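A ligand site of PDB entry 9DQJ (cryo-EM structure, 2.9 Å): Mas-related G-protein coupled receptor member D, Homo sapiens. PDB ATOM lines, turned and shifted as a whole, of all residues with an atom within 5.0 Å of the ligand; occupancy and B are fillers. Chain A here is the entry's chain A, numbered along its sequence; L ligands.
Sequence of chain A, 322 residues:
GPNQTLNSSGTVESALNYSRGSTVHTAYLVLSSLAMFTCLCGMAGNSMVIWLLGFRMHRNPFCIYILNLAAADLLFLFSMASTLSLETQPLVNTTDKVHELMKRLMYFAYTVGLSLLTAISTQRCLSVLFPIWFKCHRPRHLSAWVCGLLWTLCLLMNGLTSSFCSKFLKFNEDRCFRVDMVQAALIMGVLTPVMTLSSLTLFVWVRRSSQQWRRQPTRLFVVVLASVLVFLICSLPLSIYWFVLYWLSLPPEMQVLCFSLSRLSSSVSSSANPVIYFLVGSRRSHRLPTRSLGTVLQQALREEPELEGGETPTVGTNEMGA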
ATOM      1  N   LYS A 103     -16.997 -10.302 -21.718  1.00  0.00           N
ATOM      2  CA  LYS A 103     -17.882  -9.216 -22.132  1.00  0.00           C
ATOM      3  C   LYS A 103     -17.508  -7.921 -21.450  1.00  0.00           C
ATOM      4  O   LYS A 103     -17.475  -6.850 -22.079  1.00  0.00           O
ATOM      5  CB  LYS A 103     -19.328  -9.604 -21.824  1.00  0.00           C
ATOM      6  CG  LYS A 103     -20.352  -8.504 -22.044  1.00  0.00           C
ATOM      7  CD  LYS A 103     -21.747  -9.126 -22.155  1.00  0.00           C
ATOM      8  CE  LYS A 103     -22.829  -8.081 -22.335  1.00  0.00           C
ATOM      9  NZ  LYS A 103     -23.181  -7.400 -21.071  1.00  0.00           N
ATOM     10  N   ARG A 104     -17.204  -7.987 -20.157  1.00  0.00           N
ATOM     11  CA  ARG A 104     -16.823  -6.774 -19.453  1.00  0.00           C
ATOM     12  C   ARG A 104     -15.490  -6.220 -19.959  1.00  0.00           C
ATOM     13  O   ARG A 104     -15.340  -5.002 -20.130  1.00  0.00           O
ATOM     14  CB  ARG A 104     -16.789  -7.009 -17.956  1.00  0.00           C
ATOM     15  CG  ARG A 104     -18.173  -7.230 -17.410  1.00  0.00           C
ATOM     16  CD  ARG A 104     -19.004  -6.003 -17.692  1.00  0.00           C
ATOM     17  NE  ARG A 104     -20.339  -6.127 -17.128  1.00  0.00           N
ATOM     18  CZ  ARG A 104     -21.357  -6.670 -17.762  1.00  0.00           C
ATOM     19  NH1 ARG A 104     -21.191  -7.158 -18.981  1.00  0.00           N
ATOM     20  NH2 ARG A 104     -22.547  -6.745 -17.185  1.00  0.00           N
ATOM     21  N   TYR A 107     -16.168  -4.335 -23.219  1.00  0.00           N
ATOM     22  CA  TYR A 107     -16.702  -2.983 -23.120  1.00  0.00           C
ATOM     23  C   TYR A 107     -15.665  -2.021 -22.561  1.00  0.00           C
ATOM     24  O   TYR A 107     -15.568  -0.850 -22.999  1.00  0.00           O
ATOM     25  CB  TYR A 107     -17.974  -2.975 -22.279  1.00  0.00           C
ATOM     26  CG  TYR A 107     -19.137  -3.593 -23.000  1.00  0.00           C
ATOM     27  CD1 TYR A 107     -19.210  -3.548 -24.379  1.00  0.00           C
ATOM     28  CD2 TYR A 107     -20.153  -4.222 -22.317  1.00  0.00           C
ATOM     29  CE1 TYR A 107     -20.272  -4.114 -25.055  1.00  0.00           C
ATOM     30  CE2 TYR A 107     -21.215  -4.792 -22.985  1.00  0.00           C
ATOM     31  CZ  TYR A 107     -21.260  -4.738 -24.348  1.00  0.00           C
ATOM     32  OH  TYR A 107     -22.323  -5.294 -25.021  1.00  0.00           O
ATOM     33  N   TYR A 110     -13.349  -1.090 -25.326  1.00  0.00           N
ATOM     34  CA  TYR A 110     -14.074  -0.183 -26.208  1.00  0.00           C
ATOM     35  C   TYR A 110     -13.962   1.250 -25.731  1.00  0.00           C
ATOM     36  O   TYR A 110     -13.585   2.152 -26.496  1.00  0.00           O
ATOM     37  CB  TYR A 110     -15.525  -0.631 -26.256  1.00  0.00           C
ATOM     38  CG  TYR A 110     -16.460   0.208 -27.065  1.00  0.00           C
ATOM     39  CD1 TYR A 110     -17.400   1.017 -26.451  1.00  0.00           C
ATOM     40  CD2 TYR A 110     -16.462   0.152 -28.436  1.00  0.00           C
ATOM     41  CE1 TYR A 110     -18.282   1.770 -27.184  1.00  0.00           C
ATOM     42  CE2 TYR A 110     -17.342   0.896 -29.173  1.00  0.00           C
ATOM     43  CZ  TYR A 110     -18.243   1.702 -28.536  1.00  0.00           C
ATOM     44  OH  TYR A 110     -19.125   2.456 -29.269  1.00  0.00           O
ATOM     45  N   THR A 111     -14.266   1.490 -24.452  1.00  0.00           N
ATOM     46  CA  THR A 111     -14.208   2.848 -23.941  1.00  0.00           C
ATOM     47  C   THR A 111     -12.792   3.404 -23.993  1.00  0.00           C
ATOM     48  O   THR A 111     -12.592   4.581 -24.350  1.00  0.00           O
ATOM     49  CB  THR A 111     -14.746   2.890 -22.511  1.00  0.00           C
ATOM     50  OG1 THR A 111     -16.082   2.373 -22.505  1.00  0.00           O
ATOM     51  CG2 THR A 111     -14.785   4.297 -21.997  1.00  0.00           C
ATOM     52  N   ASN A 158     -15.851   1.585 -16.059  1.00  0.00           N
ATOM     53  CA  ASN A 158     -16.278   0.284 -16.573  1.00  0.00           C
ATOM     54  C   ASN A 158     -16.452  -0.717 -15.441  1.00  0.00           C
ATOM     55  O   ASN A 158     -17.415  -1.490 -15.443  1.00  0.00           O
ATOM     56  CB  ASN A 158     -15.277  -0.232 -17.598  1.00  0.00           C
ATOM     57  CG  ASN A 158     -15.262   0.570 -18.866  1.00  0.00           C
ATOM     58  OD1 ASN A 158     -16.244   0.602 -19.610  1.00  0.00           O
ATOM     59  ND2 ASN A 158     -14.143   1.231 -19.136  1.00  0.00           N
ATOM     60  N   THR A 161     -19.648   0.012 -13.555  1.00  0.00           N
ATOM     61  CA  THR A 161     -20.842  -0.431 -14.265  1.00  0.00           C
ATOM     62  C   THR A 161     -20.946  -1.950 -14.250  1.00  0.00           C
ATOM     63  O   THR A 161     -22.045  -2.498 -14.128  1.00  0.00           O
ATOM     64  CB  THR A 161     -20.832   0.087 -15.695  1.00  0.00           C
ATOM     65  OG1 THR A 161     -20.546   1.496 -15.691  1.00  0.00           O
ATOM     66  CG2 THR A 161     -22.196  -0.099 -16.292  1.00  0.00           C
ATOM     67  N   CYS A 165     -24.210  -3.928 -12.758  1.00  0.00           N
ATOM     68  CA  CYS A 165     -25.158  -4.344 -13.790  1.00  0.00           C
ATOM     69  C   CYS A 165     -25.103  -5.811 -14.167  1.00  0.00           C
ATOM     70  O   CYS A 165     -26.057  -6.297 -14.787  1.00  0.00           O
ATOM     71  CB  CYS A 165     -24.944  -3.512 -15.060  1.00  0.00           C
ATOM     72  SG  CYS A 165     -25.093  -1.722 -14.832  1.00  0.00           S
ATOM     73  N   SER A 166     -24.039  -6.539 -13.835  1.00  0.00           N
ATOM     74  CA  SER A 166     -23.887  -7.899 -14.316  1.00  0.00           C
ATOM     75  C   SER A 166     -24.857  -8.861 -13.619  1.00  0.00           C
ATOM     76  O   SER A 166     -25.279  -8.639 -12.480  1.00  0.00           O
ATOM     77  CB  SER A 166     -22.448  -8.358 -14.123  1.00  0.00           C
ATOM     78  OG  SER A 166     -22.271  -9.674 -14.598  1.00  0.00           O
ATOM     79  N   PHE A 171     -25.839  -6.792  -9.322  1.00  0.00           N
ATOM     80  CA  PHE A 171     -26.851  -6.040 -10.071  1.00  0.00           C
ATOM     81  C   PHE A 171     -27.793  -5.205  -9.212  1.00  0.00           C
ATOM     82  O   PHE A 171     -28.246  -5.650  -8.146  1.00  0.00           O
ATOM     83  CB  PHE A 171     -27.671  -6.995 -10.940  1.00  0.00           C
ATOM     84  CG  PHE A 171     -28.754  -6.308 -11.718  1.00  0.00           C
ATOM     85  CD1 PHE A 171     -28.453  -5.614 -12.876  1.00  0.00           C
ATOM     86  CD2 PHE A 171     -30.061  -6.328 -11.274  1.00  0.00           C
ATOM     87  CE1 PHE A 171     -29.446  -4.969 -13.590  1.00  0.00           C
ATOM     88  CE2 PHE A 171     -31.052  -5.697 -11.983  1.00  0.00           C
ATOM     89  CZ  PHE A 171     -30.750  -5.012 -13.145  1.00  0.00           C
ATOM     90  N   CYS A 176     -27.633   0.950 -11.556  1.00  0.00           N
ATOM     91  CA  CYS A 176     -27.088   0.557 -12.852  1.00  0.00           C
ATOM     92  C   CYS A 176     -27.546   1.500 -13.956  1.00  0.00           C
ATOM     93  O   CYS A 176     -26.763   1.842 -14.854  1.00  0.00           O
ATOM     94  CB  CYS A 176     -27.493  -0.879 -13.202  1.00  0.00           C
ATOM     95  SG  CYS A 176     -27.088  -1.364 -14.882  1.00  0.00           S
ATOM     96  N   ASP A 180     -25.015   3.720 -16.199  1.00  0.00           N
ATOM     97  CA  ASP A 180     -25.081   3.590 -17.654  1.00  0.00           C
ATOM     98  C   ASP A 180     -25.269   4.946 -18.322  1.00  0.00           C
ATOM     99  O   ASP A 180     -24.569   5.269 -19.285  1.00  0.00           O
ATOM    100  CB  ASP A 180     -26.214   2.643 -18.062  1.00  0.00           C
ATOM    101  CG  ASP A 180     -25.746   1.233 -18.261  1.00  0.00           C
ATOM    102  OD1 ASP A 180     -24.581   1.044 -18.661  1.00  0.00           O
ATOM    103  OD2 ASP A 180     -26.539   0.295 -18.019  1.00  0.00           O
ATOM    104  N   MET A 181     -26.208   5.744 -17.819  1.00  0.00           N
ATOM    105  CA  MET A 181     -26.389   7.069 -18.402  1.00  0.00           C
ATOM    106  C   MET A 181     -25.189   7.975 -18.147  1.00  0.00           C
ATOM    107  O   MET A 181     -24.904   8.835 -18.975  1.00  0.00           O
ATOM    108  CB  MET A 181     -27.666   7.712 -17.875  1.00  0.00           C
ATOM    109  CG  MET A 181     -28.935   7.011 -18.301  1.00  0.00           C
ATOM    110  SD  MET A 181     -29.129   7.000 -20.092  1.00  0.00           S
ATOM    111  CE  MET A 181     -28.625   5.330 -20.506  1.00  0.00           C
ATOM    112  N   GLN A 183     -22.010   7.001 -18.156  1.00  0.00           N
ATOM    113  CA  GLN A 183     -21.045   6.634 -19.190  1.00  0.00           C
ATOM    114  C   GLN A 183     -21.506   7.090 -20.577  1.00  0.00           C
ATOM    115  O   GLN A 183     -20.694   7.487 -21.410  1.00  0.00           O
ATOM    116  CB  GLN A 183     -20.795   5.127 -19.188  1.00  0.00           C
ATOM    117  CG  GLN A 183     -19.420   4.752 -19.673  1.00  0.00           C
ATOM    118  CD  GLN A 183     -19.041   3.336 -19.288  1.00  0.00           C
ATOM    119  OE1 GLN A 183     -19.901   2.532 -18.912  1.00  0.00           O
ATOM    120  NE2 GLN A 183     -17.759   3.031 -19.364  1.00  0.00           N
ATOM    121  N   ALA A 184     -22.820   7.021 -20.838  1.00  0.00           N
ATOM    122  CA  ALA A 184     -23.350   7.468 -22.113  1.00  0.00           C
ATOM    123  C   ALA A 184     -23.128   8.959 -22.295  1.00  0.00           C
ATOM    124  O   ALA A 184     -22.757   9.420 -23.379  1.00  0.00           O
ATOM    125  CB  ALA A 184     -24.840   7.154 -22.218  1.00  0.00           C
ATOM    126  N   ILE A 187     -19.375   9.445 -23.159  1.00  0.00           N
ATOM    127  CA  ILE A 187     -18.994   9.134 -24.537  1.00  0.00           C
ATOM    128  C   ILE A 187     -19.648  10.094 -25.503  1.00  0.00           C
ATOM    129  O   ILE A 187     -18.970  10.958 -26.078  1.00  0.00           O
ATOM    130  CB  ILE A 187     -19.336   7.681 -24.903  1.00  0.00           C
ATOM    131  CG1 ILE A 187     -18.277   6.738 -24.342  1.00  0.00           C
ATOM    132  CG2 ILE A 187     -19.354   7.507 -26.395  1.00  0.00           C
ATOM    133  CD1 ILE A 187     -18.501   5.311 -24.704  1.00  0.00           C
ATOM    134  N   MET A 188     -20.974  10.035 -25.622  1.00  0.00           N
ATOM    135  CA  MET A 188     -21.655  10.766 -26.677  1.00  0.00           C
ATOM    136  C   MET A 188     -21.908  12.231 -26.341  1.00  0.00           C
ATOM    137  O   MET A 188     -22.699  12.866 -27.041  1.00  0.00           O
ATOM    138  CB  MET A 188     -22.985  10.086 -27.011  1.00  0.00           C
ATOM    139  CG  MET A 188     -22.829   8.750 -27.698  1.00  0.00           C
ATOM    140  SD  MET A 188     -24.381   7.854 -27.856  1.00  0.00           S
ATOM    141  CE  MET A 188     -25.056   8.067 -26.216  1.00  0.00           C
ATOM    142  N   LEU A 238     -22.244   0.915 -31.204  1.00  0.00           N
ATOM    143  CA  LEU A 238     -22.471   0.085 -30.031  1.00  0.00           C
ATOM    144  C   LEU A 238     -23.080   0.897 -28.898  1.00  0.00           C
ATOM    145  O   LEU A 238     -24.044   0.460 -28.247  1.00  0.00           O
ATOM    146  CB  LEU A 238     -21.170  -0.580 -29.601  1.00  0.00           C
ATOM    147  CG  LEU A 238     -21.239  -1.927 -28.886  1.00  0.00           C
ATOM    148  CD1 LEU A 238     -21.562  -3.001 -29.878  1.00  0.00           C
ATOM    149  CD2 LEU A 238     -19.905  -2.236 -28.244  1.00  0.00           C
ATOM    150  N   SER A 239     -22.556   2.096 -28.676  1.00  0.00           N
ATOM    151  CA  SER A 239     -23.201   3.007 -27.733  1.00  0.00           C
ATOM    152  C   SER A 239     -24.606   3.355 -28.191  1.00  0.00           C
ATOM    153  O   SER A 239     -25.525   3.478 -27.378  1.00  0.00           O
ATOM    154  CB  SER A 239     -22.345   4.256 -27.575  1.00  0.00           C
ATOM    155  OG  SER A 239     -21.009   3.928 -27.282  1.00  0.00           O
ATOM    156  N   TRP A 242     -26.855   0.521 -27.190  1.00  0.00           N
ATOM    157  CA  TRP A 242     -27.161   0.492 -25.767  1.00  0.00           C
ATOM    158  C   TRP A 242     -28.024   1.664 -25.343  1.00  0.00           C
ATOM    159  O   TRP A 242     -28.651   1.607 -24.286  1.00  0.00           O
ATOM    160  CB  TRP A 242     -25.869   0.439 -24.964  1.00  0.00           C
ATOM    161  CG  TRP A 242     -25.434  -0.953 -24.793  1.00  0.00           C
ATOM    162  CD1 TRP A 242     -24.285  -1.506 -25.237  1.00  0.00           C
ATOM    163  CD2 TRP A 242     -26.175  -2.008 -24.165  1.00  0.00           C
ATOM    164  NE1 TRP A 242     -24.244  -2.832 -24.906  1.00  0.00           N
ATOM    165  CE2 TRP A 242     -25.393  -3.157 -24.252  1.00  0.00           C
ATOM    166  CE3 TRP A 242     -27.413  -2.068 -23.531  1.00  0.00           C
ATOM    167  CZ2 TRP A 242     -25.815  -4.378 -23.718  1.00  0.00           C
ATOM    168  CZ3 TRP A 242     -27.825  -3.272 -23.011  1.00  0.00           C
ATOM    169  CH2 TRP A 242     -27.033  -4.416 -23.106  1.00  0.00           C
ATOM    170  N   PHE A 243     -28.087   2.721 -26.142  1.00  0.00           N
ATOM    171  CA  PHE A 243     -29.072   3.754 -25.883  1.00  0.00           C
ATOM    172  C   PHE A 243     -30.460   3.338 -26.365  1.00  0.00           C
ATOM    173  O   PHE A 243     -31.462   3.590 -25.698  1.00  0.00           O
ATOM    174  CB  PHE A 243     -28.660   5.065 -26.544  1.00  0.00           C
ATOM    175  CG  PHE A 243     -29.187   6.282 -25.853  1.00  0.00           C
ATOM    176  CD1 PHE A 243     -28.488   6.840 -24.808  1.00  0.00           C
ATOM    177  CD2 PHE A 243     -30.379   6.849 -26.241  1.00  0.00           C
ATOM    178  CE1 PHE A 243     -28.969   7.949 -24.157  1.00  0.00           C
ATOM    179  CE2 PHE A 243     -30.862   7.971 -25.596  1.00  0.00           C
ATOM    180  CZ  PHE A 243     -30.161   8.521 -24.554  1.00  0.00           C
ATOM    181  N   TYR A 246     -32.534   0.770 -24.172  1.00  0.00           N
ATOM    182  CA  TYR A 246     -33.202   1.375 -23.025  1.00  0.00           C
ATOM    183  C   TYR A 246     -34.448   2.157 -23.430  1.00  0.00           C
ATOM    184  O   TYR A 246     -35.516   1.978 -22.845  1.00  0.00           O
ATOM    185  CB  TYR A 246     -32.226   2.288 -22.273  1.00  0.00           C
ATOM    186  CG  TYR A 246     -31.309   1.591 -21.303  1.00  0.00           C
ATOM    187  CD1 TYR A 246     -31.543   0.300 -20.884  1.00  0.00           C
ATOM    188  CD2 TYR A 246     -30.215   2.252 -20.782  1.00  0.00           C
ATOM    189  CE1 TYR A 246     -30.710  -0.322 -19.975  1.00  0.00           C
ATOM    190  CE2 TYR A 246     -29.375   1.653 -19.873  1.00  0.00           C
ATOM    191  CZ  TYR A 246     -29.627   0.368 -19.475  1.00  0.00           C
ATOM    192  OH  TYR A 246     -28.767  -0.225 -18.574  1.00  0.00           O
HETATM  193  C1  LIG L   1     -25.766   4.711 -24.560  1.00  0.00           C
HETATM  194  C2  LIG L   1     -19.724   1.095 -23.247  1.00  0.00           C
HETATM  195  C3  LIG L   1     -21.077  -0.087 -21.396  1.00  0.00           C
HETATM  196  C4  LIG L   1     -23.252  -1.255 -21.843  1.00  0.00           C
HETATM  197  C5  LIG L   1     -23.458  -2.743 -21.606  1.00  0.00           C
HETATM  198  C6  LIG L   1     -23.730  -3.022 -20.138  1.00  0.00           C
HETATM  199  C7  LIG L   1     -22.601  -2.458 -19.288  1.00  0.00           C
HETATM  200  C8  LIG L   1     -22.421  -0.981 -19.563  1.00  0.00           C
HETATM  201  C9  LIG L   1     -25.975  -3.294 -19.239  1.00  0.00           C
HETATM  202  C10 LIG L   1     -28.147  -3.707 -18.541  1.00  0.00           C
HETATM  203  C11 LIG L   1     -27.834  -5.040 -18.202  1.00  0.00           C
HETATM  204  C12 LIG L   1     -24.335   3.482 -23.097  1.00  0.00           C
HETATM  205  C13 LIG L   1     -28.841  -5.901 -17.672  1.00  0.00           C
HETATM  206  C14 LIG L   1     -30.111  -5.414 -17.504  1.00  0.00           C
HETATM  207  C15 LIG L   1     -30.414  -4.089 -17.845  1.00  0.00           C
HETATM  208  C16 LIG L   1     -29.455  -3.253 -18.355  1.00  0.00           C
HETATM  209  C17 LIG L   1     -26.473  -5.500 -18.409  1.00  0.00           C
HETATM  210  C18 LIG L   1     -23.940   3.074 -21.834  1.00  0.00           C
HETATM  211  C19 LIG L   1     -22.883   2.194 -21.700  1.00  0.00           C
HETATM  212  C20 LIG L   1     -22.220   1.696 -22.817  1.00  0.00           C
HETATM  213  C21 LIG L   1     -22.638   2.120 -24.075  1.00  0.00           C
HETATM  214  C22 LIG L   1     -23.684   3.005 -24.218  1.00  0.00           C
HETATM  215  C23 LIG L   1     -21.082   0.717 -22.674  1.00  0.00           C
HETATM  216  C24 LIG L   1     -20.539   0.047 -23.926  1.00  0.00           C
HETATM  217  N1  LIG L   1     -22.169  -0.744 -20.983  1.00  0.00           N
HETATM  218  N2  LIG L   1     -25.025  -2.485 -19.738  1.00  0.00           N
HETATM  219  N3  LIG L   1     -27.202  -2.837 -19.060  1.00  0.00           N
HETATM  220  N4  LIG L   1     -25.594  -4.574 -18.931  1.00  0.00           N
HETATM  221  O1  LIG L   1     -25.382   4.363 -23.231  1.00  0.00           O
HETATM  222  O2  LIG L   1     -20.067  -0.063 -20.703  1.00  0.00           O
HETATM  223  O3  LIG L   1     -26.074  -6.642 -18.144  1.00  0.00           O
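The side-chain hydroxyl of Tyr 246 lies within hydrogen-bond range of a nitrogen (N3) of the ligand (3.1 Å). The side-chain amide oxygen of Gln 183 sits close to an oxygen (O2) of the ligand (3.2 Å).
The side-chain sulfur of Cys 165 forms a disulfide with the side-chain sulfur of Cys 176, 2.0 Å away. The indole nitrogen (NE1) of Trp 242 lies within hydrogen-bond range of the side-chain hydroxyl (OH) of Tyr 107 (3.1 Å). OG1 of Thr 111 sits at hydrogen-bond distance from OD1 of Asn 158. OE1 of Gln 183 sits at hydrogen-bond distance from OG1 of Thr 161 (3.4 Å). OD1 of Asn 158 sits at hydrogen-bond distance from NE2 of Gln 183, 2.9 Å away. The side-chain hydroxyl (OG) of Ser 239 sits at hydrogen-bond distance from the side-chain hydroxyl (OH) of Tyr 110. O of Tyr 107 lies within hydrogen-bond range of OG1 of Thr 111 (3.3 Å).
O of Cys 165 sits close to O3 of the ligand, 3.4 Å away. A nitrogen (N3) of the ligand sits close to the side-chain carboxylate (OD2) of Asp 180, 3.4 Å away. NH2 of Arg 104 touches O3 of the ligand, at 3.7 Å. CE2 of Tyr 107 touches C5 of the ligand (3.3 Å). CD1 of Tyr 110 touches C2 of the ligand, 3.96 Å away. Thr 111 touches the ligand (OG1 to C2, 3.9 Å). CG2 of Thr 161 touches C8 of the ligand, 3.4 Å away. CE1 of Phe 171 touches C14 of the ligand, at 3.99 Å. Ala 184 touches the ligand (CB to O1, 3.0 Å). Met 188 touches the ligand (CE to C1, 3.8 Å). Ser 239 touches the ligand (O to C1, 3.1 Å). Trp 242 touches the ligand. Phe 243 touches the ligand (N to C1, 3.4 Å). Along chain A the residues within 4 Å of the ligand span positions 104 to 246. The nearest printed residue that does not touch the ligand is Asn 158 (4.03 Å).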
